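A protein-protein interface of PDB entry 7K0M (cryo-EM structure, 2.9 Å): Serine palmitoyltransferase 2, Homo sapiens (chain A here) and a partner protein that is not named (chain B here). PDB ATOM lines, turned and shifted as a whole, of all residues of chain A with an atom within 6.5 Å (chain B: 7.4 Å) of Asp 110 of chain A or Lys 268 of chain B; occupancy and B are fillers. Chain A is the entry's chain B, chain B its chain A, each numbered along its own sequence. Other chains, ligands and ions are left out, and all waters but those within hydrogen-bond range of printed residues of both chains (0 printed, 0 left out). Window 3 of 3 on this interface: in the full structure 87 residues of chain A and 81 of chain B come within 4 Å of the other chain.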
ATOM      1  N   ARG A 105      13.685 -16.299  20.377  1.00  0.00           N
ATOM      2  CA  ARG A 105      14.837 -17.154  20.615  1.00  0.00           C
ATOM      3  C   ARG A 105      16.012 -16.721  19.747  1.00  0.00           C
ATOM      4  O   ARG A 105      15.840 -16.158  18.662  1.00  0.00           O
ATOM      5  CB  ARG A 105      14.487 -18.616  20.341  1.00  0.00           C
ATOM      6  CG  ARG A 105      13.776 -18.852  19.026  1.00  0.00           C
ATOM      7  CD  ARG A 105      13.136 -20.226  18.995  1.00  0.00           C
ATOM      8  NE  ARG A 105      14.076 -21.281  19.357  1.00  0.00           N
ATOM      9  CZ  ARG A 105      14.686 -22.071  18.480  1.00  0.00           C
ATOM     10  NH1 ARG A 105      14.456 -21.926  17.184  1.00  0.00           N
ATOM     11  NH2 ARG A 105      15.525 -23.007  18.900  1.00  0.00           N
ATOM     12  N   GLU A 106      17.222 -16.987  20.243  1.00  0.00           N
ATOM     13  CA  GLU A 106      18.426 -16.494  19.581  1.00  0.00           C
ATOM     14  C   GLU A 106      18.587 -17.075  18.183  1.00  0.00           C
ATOM     15  O   GLU A 106      19.170 -16.427  17.308  1.00  0.00           O
ATOM     16  CB  GLU A 106      19.655 -16.809  20.430  1.00  0.00           C
ATOM     17  CG  GLU A 106      19.674 -16.103  21.773  1.00  0.00           C
ATOM     18  CD  GLU A 106      19.798 -14.599  21.640  1.00  0.00           C
ATOM     19  OE1 GLU A 106      20.451 -14.136  20.681  1.00  0.00           O
ATOM     20  OE2 GLU A 106      19.242 -13.878  22.495  1.00  0.00           O
ATOM     21  N   GLU A 107      18.083 -18.287  17.950  1.00  0.00           N
ATOM     22  CA  GLU A 107      18.213 -18.912  16.641  1.00  0.00           C
ATOM     23  C   GLU A 107      17.336 -18.260  15.581  1.00  0.00           C
ATOM     24  O   GLU A 107      17.507 -18.559  14.396  1.00  0.00           O
ATOM     25  CB  GLU A 107      17.882 -20.401  16.736  1.00  0.00           C
ATOM     26  CG  GLU A 107      18.901 -21.217  17.510  1.00  0.00           C
ATOM     27  CD  GLU A 107      18.638 -21.222  19.001  1.00  0.00           C
ATOM     28  OE1 GLU A 107      17.731 -20.491  19.449  1.00  0.00           O
ATOM     29  OE2 GLU A 107      19.336 -21.958  19.728  1.00  0.00           O
ATOM     30  N   GLN A 108      16.410 -17.383  15.970  1.00  0.00           N
ATOM     31  CA  GLN A 108      15.488 -16.749  15.038  1.00  0.00           C
ATOM     32  C   GLN A 108      15.616 -15.229  15.062  1.00  0.00           C
ATOM     33  O   GLN A 108      14.645 -14.514  14.809  1.00  0.00           O
ATOM     34  CB  GLN A 108      14.051 -17.168  15.335  1.00  0.00           C
ATOM     35  CG  GLN A 108      13.824 -18.662  15.255  1.00  0.00           C
ATOM     36  CD  GLN A 108      12.378 -19.039  15.472  1.00  0.00           C
ATOM     37  OE1 GLN A 108      11.525 -18.177  15.673  1.00  0.00           O
ATOM     38  NE2 GLN A 108      12.091 -20.333  15.436  1.00  0.00           N
ATOM     39  N   LYS A 109      16.812 -14.722  15.369  1.00  0.00           N
ATOM     40  CA  LYS A 109      17.035 -13.281  15.363  1.00  0.00           C
ATOM     41  C   LYS A 109      16.998 -12.695  13.959  1.00  0.00           C
ATOM     42  O   LYS A 109      16.708 -11.504  13.806  1.00  0.00           O
ATOM     43  CB  LYS A 109      18.372 -12.952  16.024  1.00  0.00           C
ATOM     44  CG  LYS A 109      18.369 -13.094  17.535  1.00  0.00           C
ATOM     45  CD  LYS A 109      17.267 -12.261  18.165  1.00  0.00           C
ATOM     46  CE  LYS A 109      17.279 -12.387  19.679  1.00  0.00           C
ATOM     47  NZ  LYS A 109      16.262 -11.507  20.317  1.00  0.00           N
ATOM     48  N   ASP A 110      17.289 -13.495  12.936  1.00  0.00           N
ATOM     49  CA  ASP A 110      17.264 -13.023  11.560  1.00  0.00           C
ATOM     50  C   ASP A 110      15.905 -13.180  10.888  1.00  0.00           C
ATOM     51  O   ASP A 110      15.744 -12.735   9.747  1.00  0.00           O
ATOM     52  CB  ASP A 110      18.346 -13.739  10.740  1.00  0.00           C
ATOM     53  CG  ASP A 110      18.130 -15.238  10.657  1.00  0.00           C
ATOM     54  OD1 ASP A 110      17.169 -15.748  11.265  1.00  0.00           O
ATOM     55  OD2 ASP A 110      18.932 -15.912   9.977  1.00  0.00           O
ATOM     56  N   PHE A 111      14.932 -13.795  11.555  1.00  0.00           N
ATOM     57  CA  PHE A 111      13.585 -13.851  11.011  1.00  0.00           C
ATOM     58  C   PHE A 111      12.937 -12.472  11.067  1.00  0.00           C
ATOM     59  O   PHE A 111      13.347 -11.592  11.827  1.00  0.00           O
ATOM     60  CB  PHE A 111      12.710 -14.843  11.784  1.00  0.00           C
ATOM     61  CG  PHE A 111      13.039 -16.293  11.545  1.00  0.00           C
ATOM     62  CD1 PHE A 111      14.231 -16.677  10.962  1.00  0.00           C
ATOM     63  CD2 PHE A 111      12.134 -17.274  11.901  1.00  0.00           C
ATOM     64  CE1 PHE A 111      14.516 -18.012  10.754  1.00  0.00           C
ATOM     65  CE2 PHE A 111      12.413 -18.606  11.690  1.00  0.00           C
ATOM     66  CZ  PHE A 111      13.605 -18.975  11.115  1.00  0.00           C
ATOM     67  N   VAL A 112      11.906 -12.288  10.241  1.00  0.00           N
ATOM     68  CA  VAL A 112      11.084 -11.092  10.350  1.00  0.00           C
ATOM     69  C   VAL A 112      10.393 -11.091  11.706  1.00  0.00           C
ATOM     70  O   VAL A 112       9.938 -12.135  12.191  1.00  0.00           O
ATOM     71  CB  VAL A 112      10.066 -11.030   9.200  1.00  0.00           C
ATOM     72  CG1 VAL A 112       9.341  -9.699   9.203  1.00  0.00           C
ATOM     73  CG2 VAL A 112      10.758 -11.260   7.874  1.00  0.00           C
ATOM     74  N   LEU B 221       8.753 -21.694  -2.112  1.00  0.00           N
ATOM     75  CA  LEU B 221       9.662 -20.863  -1.331  1.00  0.00           C
ATOM     76  C   LEU B 221      10.691 -20.175  -2.222  1.00  0.00           C
ATOM     77  O   LEU B 221      11.045 -19.012  -1.989  1.00  0.00           O
ATOM     78  CB  LEU B 221      10.348 -21.705  -0.257  1.00  0.00           C
ATOM     79  CG  LEU B 221       9.459 -22.162   0.901  1.00  0.00           C
ATOM     80  CD1 LEU B 221      10.151 -23.232   1.720  1.00  0.00           C
ATOM     81  CD2 LEU B 221       9.088 -20.984   1.777  1.00  0.00           C
ATOM     82  N   THR B 238       7.328  -8.547   5.644  1.00  0.00           N
ATOM     83  CA  THR B 238       6.421  -9.624   5.271  1.00  0.00           C
ATOM     84  C   THR B 238       6.823 -10.895   6.003  1.00  0.00           C
ATOM     85  O   THR B 238       7.976 -11.329   5.912  1.00  0.00           O
ATOM     86  CB  THR B 238       6.432  -9.856   3.760  1.00  0.00           C
ATOM     87  OG1 THR B 238       5.726  -8.795   3.108  1.00  0.00           O
ATOM     88  CG2 THR B 238       5.771 -11.177   3.416  1.00  0.00           C
ATOM     89  N   ARG B 239       5.875 -11.487   6.722  1.00  0.00           N
ATOM     90  CA  ARG B 239       6.111 -12.692   7.499  1.00  0.00           C
ATOM     91  C   ARG B 239       5.587 -13.910   6.752  1.00  0.00           C
ATOM     92  O   ARG B 239       4.616 -13.828   5.998  1.00  0.00           O
ATOM     93  CB  ARG B 239       5.448 -12.585   8.873  1.00  0.00           C
ATOM     94  CG  ARG B 239       6.018 -11.472   9.732  1.00  0.00           C
ATOM     95  CD  ARG B 239       4.941 -10.762  10.529  1.00  0.00           C
ATOM     96  NE  ARG B 239       5.450  -9.550  11.164  1.00  0.00           N
ATOM     97  CZ  ARG B 239       5.305  -8.327  10.665  1.00  0.00           C
ATOM     98  NH1 ARG B 239       4.659  -8.146   9.523  1.00  0.00           N
ATOM     99  NH2 ARG B 239       5.802  -7.283  11.310  1.00  0.00           N
ATOM    100  N   ARG B 240       6.246 -15.048   6.966  1.00  0.00           N
ATOM    101  CA  ARG B 240       5.951 -16.271   6.233  1.00  0.00           C
ATOM    102  C   ARG B 240       5.668 -17.402   7.208  1.00  0.00           C
ATOM    103  O   ARG B 240       6.441 -17.627   8.146  1.00  0.00           O
ATOM    104  CB  ARG B 240       7.113 -16.645   5.311  1.00  0.00           C
ATOM    105  CG  ARG B 240       7.418 -15.596   4.261  1.00  0.00           C
ATOM    106  CD  ARG B 240       8.880 -15.629   3.859  1.00  0.00           C
ATOM    107  NE  ARG B 240       9.229 -14.495   3.011  1.00  0.00           N
ATOM    108  CZ  ARG B 240       9.673 -13.330   3.470  1.00  0.00           C
ATOM    109  NH1 ARG B 240       9.825 -13.146   4.773  1.00  0.00           N
ATOM    110  NH2 ARG B 240       9.966 -12.352   2.628  1.00  0.00           N
ATOM    111  N   PHE B 241       4.569 -18.119   6.977  1.00  0.00           N
ATOM    112  CA  PHE B 241       4.142 -19.206   7.843  1.00  0.00           C
ATOM    113  C   PHE B 241       3.920 -20.468   7.023  1.00  0.00           C
ATOM    114  O   PHE B 241       3.572 -20.408   5.841  1.00  0.00           O
ATOM    115  CB  PHE B 241       2.852 -18.850   8.598  1.00  0.00           C
ATOM    116  CG  PHE B 241       2.965 -17.620   9.450  1.00  0.00           C
ATOM    117  CD1 PHE B 241       3.509 -17.688  10.719  1.00  0.00           C
ATOM    118  CD2 PHE B 241       2.519 -16.397   8.985  1.00  0.00           C
ATOM    119  CE1 PHE B 241       3.611 -16.559  11.503  1.00  0.00           C
ATOM    120  CE2 PHE B 241       2.620 -15.266   9.766  1.00  0.00           C
ATOM    121  CZ  PHE B 241       3.166 -15.349  11.026  1.00  0.00           C
ATOM    122  N   ILE B 242       4.128 -21.614   7.666  1.00  0.00           N
ATOM    123  CA  ILE B 242       3.905 -22.928   7.077  1.00  0.00           C
ATOM    124  C   ILE B 242       2.999 -23.685   8.036  1.00  0.00           C
ATOM    125  O   ILE B 242       3.409 -24.003   9.156  1.00  0.00           O
ATOM    126  CB  ILE B 242       5.215 -23.695   6.855  1.00  0.00           C
ATOM    127  CG1 ILE B 242       6.112 -22.961   5.859  1.00  0.00           C
ATOM    128  CG2 ILE B 242       4.933 -25.109   6.385  1.00  0.00           C
ATOM    129  CD1 ILE B 242       7.494 -23.558   5.745  1.00  0.00           C
ATOM    130  N   LYS B 262      14.212 -28.068   8.197  1.00  0.00           N
ATOM    131  CA  LYS B 262      15.306 -27.583   7.361  1.00  0.00           C
ATOM    132  C   LYS B 262      14.839 -26.454   6.450  1.00  0.00           C
ATOM    133  O   LYS B 262      15.528 -25.437   6.305  1.00  0.00           O
ATOM    134  CB  LYS B 262      15.888 -28.725   6.531  1.00  0.00           C
ATOM    135  CG  LYS B 262      16.572 -29.809   7.336  1.00  0.00           C
ATOM    136  CD  LYS B 262      16.906 -30.999   6.451  1.00  0.00           C
ATOM    137  CE  LYS B 262      17.371 -32.189   7.270  1.00  0.00           C
ATOM    138  NZ  LYS B 262      17.432 -33.427   6.447  1.00  0.00           N
ATOM    139  N   LEU B 263      13.666 -26.613   5.835  1.00  0.00           N
ATOM    140  CA  LEU B 263      13.141 -25.571   4.961  1.00  0.00           C
ATOM    141  C   LEU B 263      12.857 -24.291   5.735  1.00  0.00           C
ATOM    142  O   LEU B 263      13.082 -23.187   5.227  1.00  0.00           O
ATOM    143  CB  LEU B 263      11.881 -26.067   4.256  1.00  0.00           C
ATOM    144  CG  LEU B 263      12.062 -26.586   2.831  1.00  0.00           C
ATOM    145  CD1 LEU B 263      13.014 -27.766   2.809  1.00  0.00           C
ATOM    146  CD2 LEU B 263      10.724 -26.977   2.245  1.00  0.00           C
ATOM    147  N   LYS B 264      12.353 -24.418   6.965  1.00  0.00           N
ATOM    148  CA  LYS B 264      12.126 -23.242   7.796  1.00  0.00           C
ATOM    149  C   LYS B 264      13.427 -22.501   8.056  1.00  0.00           C
ATOM    150  O   LYS B 264      13.528 -21.292   7.819  1.00  0.00           O
ATOM    151  CB  LYS B 264      11.484 -23.637   9.125  1.00  0.00           C
ATOM    152  CG  LYS B 264      11.728 -22.596  10.210  1.00  0.00           C
ATOM    153  CD  LYS B 264      10.854 -22.776  11.430  1.00  0.00           C
ATOM    154  CE  LYS B 264      11.605 -23.460  12.547  1.00  0.00           C
ATOM    155  NZ  LYS B 264      11.017 -23.104  13.862  1.00  0.00           N
ATOM    156  N   TYR B 265      14.443 -23.216   8.538  1.00  0.00           N
ATOM    157  CA  TYR B 265      15.691 -22.551   8.887  1.00  0.00           C
ATOM    158  C   TYR B 265      16.445 -22.054   7.662  1.00  0.00           C
ATOM    159  O   TYR B 265      17.305 -21.179   7.795  1.00  0.00           O
ATOM    160  CB  TYR B 265      16.572 -23.481   9.716  1.00  0.00           C
ATOM    161  CG  TYR B 265      16.215 -23.474  11.184  1.00  0.00           C
ATOM    162  CD1 TYR B 265      16.238 -22.296  11.913  1.00  0.00           C
ATOM    163  CD2 TYR B 265      15.851 -24.641  11.837  1.00  0.00           C
ATOM    164  CE1 TYR B 265      15.911 -22.280  13.254  1.00  0.00           C
ATOM    165  CE2 TYR B 265      15.523 -24.635  13.177  1.00  0.00           C
ATOM    166  CZ  TYR B 265      15.555 -23.452  13.880  1.00  0.00           C
ATOM    167  OH  TYR B 265      15.230 -23.438  15.217  1.00  0.00           O
ATOM    168  N   LYS B 266      16.142 -22.581   6.476  1.00  0.00           N
ATOM    169  CA  LYS B 266      16.796 -22.123   5.260  1.00  0.00           C
ATOM    170  C   LYS B 266      16.035 -21.011   4.546  1.00  0.00           C
ATOM    171  O   LYS B 266      16.636 -20.297   3.738  1.00  0.00           O
ATOM    172  CB  LYS B 266      17.010 -23.308   4.305  1.00  0.00           C
ATOM    173  CG  LYS B 266      17.997 -23.042   3.178  1.00  0.00           C
ATOM    174  CD  LYS B 266      18.452 -24.333   2.514  1.00  0.00           C
ATOM    175  CE  LYS B 266      17.421 -24.867   1.539  1.00  0.00           C
ATOM    176  NZ  LYS B 266      17.393 -24.075   0.281  1.00  0.00           N
ATOM    177  N   TYR B 267      14.743 -20.829   4.829  1.00  0.00           N
ATOM    178  CA  TYR B 267      13.963 -19.788   4.173  1.00  0.00           C
ATOM    179  C   TYR B 267      13.291 -18.812   5.130  1.00  0.00           C
ATOM    180  O   TYR B 267      12.526 -17.956   4.670  1.00  0.00           O
ATOM    181  CB  TYR B 267      12.895 -20.406   3.262  1.00  0.00           C
ATOM    182  CG  TYR B 267      13.457 -21.152   2.077  1.00  0.00           C
ATOM    183  CD1 TYR B 267      13.974 -22.430   2.217  1.00  0.00           C
ATOM    184  CD2 TYR B 267      13.483 -20.570   0.818  1.00  0.00           C
ATOM    185  CE1 TYR B 267      14.485 -23.112   1.138  1.00  0.00           C
ATOM    186  CE2 TYR B 267      13.997 -21.245  -0.268  1.00  0.00           C
ATOM    187  CZ  TYR B 267      14.499 -22.517  -0.101  1.00  0.00           C
ATOM    188  OH  TYR B 267      15.014 -23.197  -1.178  1.00  0.00           O
ATOM    189  N   LYS B 268      13.550 -18.911   6.435  1.00  0.00           N
ATOM    190  CA  LYS B 268      13.025 -17.978   7.434  1.00  0.00           C
ATOM    191  C   LYS B 268      11.495 -17.917   7.393  1.00  0.00           C
ATOM    192  O   LYS B 268      10.894 -16.871   7.140  1.00  0.00           O
ATOM    193  CB  LYS B 268      13.629 -16.578   7.254  1.00  0.00           C
ATOM    194  CG  LYS B 268      15.076 -16.543   6.781  1.00  0.00           C
ATOM    195  CD  LYS B 268      16.033 -17.028   7.849  1.00  0.00           C
ATOM    196  CE  LYS B 268      17.445 -17.146   7.310  1.00  0.00           C
ATOM    197  NZ  LYS B 268      18.337 -17.863   8.263  1.00  0.00           N
ATOM    198  N   ALA B 269      10.867 -19.062   7.655  1.00  0.00           N
ATOM    199  CA  ALA B 269       9.412 -19.167   7.652  1.00  0.00           C
ATOM    200  C   ALA B 269       8.971 -20.000   8.845  1.00  0.00           C
ATOM    201  O   ALA B 269       9.361 -21.162   8.963  1.00  0.00           O
ATOM    202  CB  ALA B 269       8.905 -19.789   6.348  1.00  0.00           C
ATOM    203  N   ARG B 270       8.141 -19.418   9.707  1.00  0.00           N
ATOM    204  CA  ARG B 270       7.727 -20.086  10.934  1.00  0.00           C
ATOM    205  C   ARG B 270       6.789 -21.253  10.632  1.00  0.00           C
ATOM    206  O   ARG B 270       6.269 -21.389   9.527  1.00  0.00           O
ATOM    207  CB  ARG B 270       7.062 -19.085  11.873  1.00  0.00           C
ATOM    208  CG  ARG B 270       8.005 -17.989  12.324  1.00  0.00           C
ATOM    209  CD  ARG B 270       7.313 -16.957  13.185  1.00  0.00           C
ATOM    210  NE  ARG B 270       8.275 -16.036  13.781  1.00  0.00           N
ATOM    211  CZ  ARG B 270       8.803 -14.997  13.146  1.00  0.00           C
ATOM    212  NH1 ARG B 270       9.670 -14.213  13.766  1.00  0.00           N
ATOM    213  NH2 ARG B 270       8.462 -14.739  11.892  1.00  0.00           N
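Of chain A, only Asp 110 and Phe 111 come within 4 Å of Lys 268 of chain B. Of the printed residues of chain B, Val 112 of chain A touches Thr 238, Arg 239, Arg 240 and Arg 270. Of the printed residues of chain A, Thr 238 of chain B touches Val 112. Printed residues of chain A within 4 Å of Tyr 265 of chain B: Arg 105 (2.6 Å). Ala 269 of chain B touches none of the printed residues of chain A. Glu 107 of chain A touches none of the printed residues of chain B. The nearest printed residue of chain B that does not touch Val 112 of chain A is Lys 268 of chain B (5.5 Å).
Of the 15 printed residues of chain B, 7 touch a printed residue of chain A. Of the 8 printed residues of chain A, 5 touch a printed residue of chain B. Hydrophobic or aromatic side chains of chain A within 4 Å of the printed part of chain B: Phe 111 and Val 112. Among the printed residues, 9 pairs touch across the chains. Among the printed residues, Asp or Glu carboxylates within 4 Å of a Lys or Arg side-chain nitrogen of the other chain: Asp 110 of chain A with Lys 268 of chain B (2.7 Å).
The backbone carbonyl oxygen of Thr 238 of chain B sits at hydrogen-bond distance from the guanidinium group of Arg 240 of chain B, at 2.8 Å. The backbone carbonyl oxygen (O) of Arg 240 of chain B is in hydrogen-bond range of the backbone NH (N) of Arg 270 of chain B, at 2.9 Å. N of Ile 242 of chain B sits at hydrogen-bond distance from O of Arg 270 of chain B. The backbone carbonyl oxygen of Lys 264 of chain B is in hydrogen-bond range of the backbone NH of Ala 269 of chain B (3.5 Å). NH2 of Arg 105 of chain A is in salt-bridge range of OE1 of Glu 107 of chain A (3.4 Å). NH1 of Arg 105 of chain A sits close to NE2 of Gln 108 of chain A (3.3 Å).
Lys 268 of chain B touches Phe 111 of chain A (CD to CE1, 3.4 Å). Arg 270 of chain B touches Phe 111 of chain A (NH1 to CB, 3.7 Å). Thr 238 of chain B touches Val 112 of chain A. Val 112 of chain A touches Arg 239 of chain B. Arg 240 of chain B touches Val 112 of chain A.
The side-chain amino group of Lys 264 of chain B lies close to the side-chain amide nitrogen of Gln 108 of chain A, at 3.4 Å. The guanidinium group (NH1) of Arg 105 of chain A sits at hydrogen-bond distance from the side-chain hydroxyl (OH) of Tyr 265 of chain B, at 2.6 Å. The side-chain carboxylate of Asp 110 of chain A is in salt-bridge range of the side-chain amino group of Lys 268 of chain B (2.7 Å). The guanidinium group (NH1) of Arg 270 of chain B is in hydrogen-bond range of the backbone carbonyl oxygen (O) of Val 112 of chain A.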
